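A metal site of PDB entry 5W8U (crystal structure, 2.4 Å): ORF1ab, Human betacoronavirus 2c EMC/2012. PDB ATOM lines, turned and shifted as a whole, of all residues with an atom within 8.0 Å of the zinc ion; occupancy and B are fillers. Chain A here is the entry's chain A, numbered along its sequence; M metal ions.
The side-chain sulfur (SG) of Cys 191 sits close to the backbone NH (N) of Val 193.
N of Gly 230 lies close to SG of Cys 228 (3.4 Å).
The zinc ion is bound by SG of Cys 191 (2.2 Å), SG of Cys 228 (2.3 Å), SG of Cys 194 (2.3 Å) and SG of Cys 226 (2.4 Å).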
ATOM      1  N   TRP A 190      22.412 -10.250   9.688  1.00  0.00           N
ATOM      2  CA  TRP A 190      22.751  -8.840   9.541  1.00  0.00           C
ATOM      3  C   TRP A 190      21.757  -8.152   8.615  1.00  0.00           C
ATOM      4  O   TRP A 190      21.157  -8.777   7.738  1.00  0.00           O
ATOM      5  CB  TRP A 190      24.192  -8.648   9.040  1.00  0.00           C
ATOM      6  CG  TRP A 190      24.508  -9.152   7.664  1.00  0.00           C
ATOM      7  CD1 TRP A 190      24.524  -8.419   6.505  1.00  0.00           C
ATOM      8  CD2 TRP A 190      24.897 -10.483   7.295  1.00  0.00           C
ATOM      9  NE1 TRP A 190      24.878  -9.223   5.434  1.00  0.00           N
ATOM     10  CE2 TRP A 190      25.112 -10.489   5.894  1.00  0.00           C
ATOM     11  CE3 TRP A 190      25.067 -11.677   8.015  1.00  0.00           C
ATOM     12  CZ2 TRP A 190      25.497 -11.643   5.215  1.00  0.00           C
ATOM     13  CZ3 TRP A 190      25.442 -12.813   7.328  1.00  0.00           C
ATOM     14  CH2 TRP A 190      25.660 -12.786   5.933  1.00  0.00           C
ATOM     15  N   CYS A 191      21.589  -6.855   8.851  1.00  0.00           N
ATOM     16  CA  CYS A 191      20.751  -5.968   8.065  1.00  0.00           C
ATOM     17  C   CYS A 191      21.454  -4.620   7.998  1.00  0.00           C
ATOM     18  O   CYS A 191      21.902  -4.119   9.040  1.00  0.00           O
ATOM     19  CB  CYS A 191      19.357  -5.828   8.693  1.00  0.00           C
ATOM     20  SG  CYS A 191      18.436  -4.337   8.278  1.00  0.00           S
ATOM     21  N   ASN A 192      21.567  -4.055   6.795  1.00  0.00           N
ATOM     22  CA  ASN A 192      22.380  -2.853   6.619  1.00  0.00           C
ATOM     23  C   ASN A 192      21.882  -1.682   7.454  1.00  0.00           C
ATOM     24  O   ASN A 192      22.658  -0.735   7.685  1.00  0.00           O
ATOM     25  CB  ASN A 192      22.425  -2.456   5.144  1.00  0.00           C
ATOM     26  CG  ASN A 192      23.251  -3.421   4.307  1.00  0.00           C
ATOM     27  OD1 ASN A 192      24.141  -4.085   4.825  1.00  0.00           O
ATOM     28  ND2 ASN A 192      22.954  -3.480   3.014  1.00  0.00           N
ATOM     29  N   VAL A 193      20.641  -1.707   7.908  1.00  0.00           N
ATOM     30  CA  VAL A 193      20.094  -0.648   8.752  1.00  0.00           C
ATOM     31  C   VAL A 193      20.100  -1.038  10.217  1.00  0.00           C
ATOM     32  O   VAL A 193      20.416  -0.217  11.084  1.00  0.00           O
ATOM     33  CB  VAL A 193      18.676  -0.276   8.279  1.00  0.00           C
ATOM     34  CG1 VAL A 193      18.184   0.981   8.998  1.00  0.00           C
ATOM     35  CG2 VAL A 193      18.655  -0.059   6.773  1.00  0.00           C
ATOM     36  N   CYS A 194      19.755  -2.297  10.524  1.00  0.00           N
ATOM     37  CA  CYS A 194      19.596  -2.736  11.905  1.00  0.00           C
ATOM     38  C   CYS A 194      20.911  -3.190  12.548  1.00  0.00           C
ATOM     39  O   CYS A 194      21.027  -3.127  13.773  1.00  0.00           O
ATOM     40  CB  CYS A 194      18.576  -3.881  11.978  1.00  0.00           C
ATOM     41  SG  CYS A 194      16.933  -3.421  11.421  1.00  0.00           S
ATOM     42  N   GLY A 195      21.871  -3.648  11.766  1.00  0.00           N
ATOM     43  CA  GLY A 195      23.138  -4.110  12.285  1.00  0.00           C
ATOM     44  C   GLY A 195      23.274  -5.620  12.188  1.00  0.00           C
ATOM     45  O   GLY A 195      22.529  -6.302  11.466  1.00  0.00           O
ATOM     46  N   TYR A 224      15.828 -12.529   3.409  1.00  0.00           N
ATOM     47  CA  TYR A 224      14.402 -12.471   3.708  1.00  0.00           C
ATOM     48  C   TYR A 224      14.126 -11.109   4.332  1.00  0.00           C
ATOM     49  O   TYR A 224      15.046 -10.397   4.738  1.00  0.00           O
ATOM     50  CB  TYR A 224      13.970 -13.627   4.621  1.00  0.00           C
ATOM     51  CG  TYR A 224      14.783 -13.721   5.895  1.00  0.00           C
ATOM     52  CD1 TYR A 224      14.303 -13.225   7.100  1.00  0.00           C
ATOM     53  CD2 TYR A 224      16.044 -14.310   5.891  1.00  0.00           C
ATOM     54  CE1 TYR A 224      15.049 -13.307   8.259  1.00  0.00           C
ATOM     55  CE2 TYR A 224      16.802 -14.398   7.045  1.00  0.00           C
ATOM     56  CZ  TYR A 224      16.298 -13.898   8.227  1.00  0.00           C
ATOM     57  OH  TYR A 224      17.061 -13.988   9.373  1.00  0.00           O
ATOM     58  N   VAL A 225      12.842 -10.756   4.417  1.00  0.00           N
ATOM     59  CA  VAL A 225      12.462  -9.424   4.859  1.00  0.00           C
ATOM     60  C   VAL A 225      12.808  -9.235   6.332  1.00  0.00           C
ATOM     61  O   VAL A 225      12.611 -10.137   7.163  1.00  0.00           O
ATOM     62  CB  VAL A 225      10.974  -9.166   4.578  1.00  0.00           C
ATOM     63  CG1 VAL A 225      10.068 -10.017   5.466  1.00  0.00           C
ATOM     64  CG2 VAL A 225      10.644  -7.678   4.729  1.00  0.00           C
ATOM     65  N   CYS A 226      13.366  -8.079   6.651  1.00  0.00           N
ATOM     66  CA  CYS A 226      13.697  -7.688   8.008  1.00  0.00           C
ATOM     67  C   CYS A 226      12.522  -6.971   8.665  1.00  0.00           C
ATOM     68  O   CYS A 226      11.604  -6.499   8.001  1.00  0.00           O
ATOM     69  CB  CYS A 226      14.936  -6.778   8.012  1.00  0.00           C
ATOM     70  SG  CYS A 226      15.631  -6.512   9.643  1.00  0.00           S
ATOM     71  N   GLN A 227      12.574  -6.881  10.000  1.00  0.00           N
ATOM     72  CA  GLN A 227      11.507  -6.197  10.728  1.00  0.00           C
ATOM     73  C   GLN A 227      11.413  -4.727  10.332  1.00  0.00           C
ATOM     74  O   GLN A 227      10.338  -4.125  10.437  1.00  0.00           O
ATOM     75  CB  GLN A 227      11.708  -6.333  12.240  1.00  0.00           C
ATOM     76  CG  GLN A 227      10.448  -6.076  13.048  1.00  0.00           C
ATOM     77  CD  GLN A 227      10.627  -6.268  14.560  1.00  0.00           C
ATOM     78  OE1 GLN A 227      11.364  -7.150  15.000  1.00  0.00           O
ATOM     79  NE2 GLN A 227       9.957  -5.446  15.344  1.00  0.00           N
ATOM     80  N   CYS A 228      12.510  -4.135   9.863  1.00  0.00           N
ATOM     81  CA  CYS A 228      12.513  -2.760   9.386  1.00  0.00           C
ATOM     82  C   CYS A 228      11.963  -2.619   7.972  1.00  0.00           C
ATOM     83  O   CYS A 228      11.820  -1.483   7.493  1.00  0.00           O
ATOM     84  CB  CYS A 228      13.931  -2.186   9.432  1.00  0.00           C
ATOM     85  SG  CYS A 228      15.080  -2.911   8.230  1.00  0.00           S
ATOM     86  N   GLY A 229      11.663  -3.719   7.294  1.00  0.00           N
ATOM     87  CA  GLY A 229      11.242  -3.664   5.905  1.00  0.00           C
ATOM     88  C   GLY A 229      12.339  -3.903   4.887  1.00  0.00           C
ATOM     89  O   GLY A 229      12.021  -4.155   3.712  1.00  0.00           O
ATOM     90  N   GLY A 230      13.604  -3.824   5.285  1.00  0.00           N
ATOM     91  CA  GLY A 230      14.716  -4.082   4.392  1.00  0.00           C
ATOM     92  C   GLY A 230      14.952  -5.558   4.168  1.00  0.00           C
ATOM     93  O   GLY A 230      14.098  -6.411   4.458  1.00  0.00           O
ATOM     94  N   GLU A 231      16.126  -5.871   3.657  1.00  0.00           N
ATOM     95  CA  GLU A 231      16.490  -7.257   3.423  1.00  0.00           C
ATOM     96  C   GLU A 231      17.500  -7.676   4.485  1.00  0.00           C
ATOM     97  O   GLU A 231      18.521  -7.004   4.689  1.00  0.00           O
ATOM     98  CB  GLU A 231      17.024  -7.454   2.003  1.00  0.00           C
ATOM     99  CG  GLU A 231      15.841  -7.695   1.055  1.00  0.00           C
ATOM    100  CD  GLU A 231      16.117  -8.305  -0.297  1.00  0.00           C
ATOM    101  OE1 GLU A 231      15.186  -8.952  -0.858  1.00  0.00           O
ATOM    102  OE2 GLU A 231      17.269  -8.133  -0.803  1.00  0.00           O
ATOM    103  N   ARG A 232      17.175  -8.738   5.193  1.00  0.00           N
ATOM    104  CA  ARG A 232      18.019  -9.303   6.225  1.00  0.00           C
ATOM    105  C   ARG A 232      18.705 -10.546   5.680  1.00  0.00           C
ATOM    106  O   ARG A 232      18.151 -11.269   4.845  1.00  0.00           O
ATOM    107  CB  ARG A 232      17.200  -9.643   7.463  1.00  0.00           C
ATOM    108  CG  ARG A 232      18.035 -10.156   8.627  1.00  0.00           C
ATOM    109  CD  ARG A 232      17.275 -10.018   9.946  1.00  0.00           C
ATOM    110  NE  ARG A 232      15.934 -10.586   9.846  1.00  0.00           N
ATOM    111  CZ  ARG A 232      15.006 -10.507  10.799  1.00  0.00           C
ATOM    112  NH1 ARG A 232      15.278  -9.868  11.941  1.00  0.00           N
ATOM    113  NH2 ARG A 232      13.814 -11.061  10.623  1.00  0.00           N
ATOM    114  N   HIS A 233      19.924 -10.780   6.140  1.00  0.00           N
ATOM    115  CA  HIS A 233      20.702 -11.927   5.735  1.00  0.00           C
ATOM    116  C   HIS A 233      21.028 -12.788   6.943  1.00  0.00           C
ATOM    117  O   HIS A 233      21.088 -12.305   8.078  1.00  0.00           O
ATOM    118  CB  HIS A 233      21.980 -11.498   5.026  1.00  0.00           C
ATOM    119  CG  HIS A 233      21.743 -10.512   3.928  1.00  0.00           C
ATOM    120  ND1 HIS A 233      21.406 -10.883   2.643  1.00  0.00           N
ATOM    121  CD2 HIS A 233      21.769  -9.155   3.931  1.00  0.00           C
ATOM    122  CE1 HIS A 233      21.251  -9.799   1.896  1.00  0.00           C
ATOM    123  NE2 HIS A 233      21.465  -8.738   2.653  1.00  0.00           N
HETATM  124 ZN    ZN M   1      16.481  -4.339   9.326  1.00  0.00          ZN
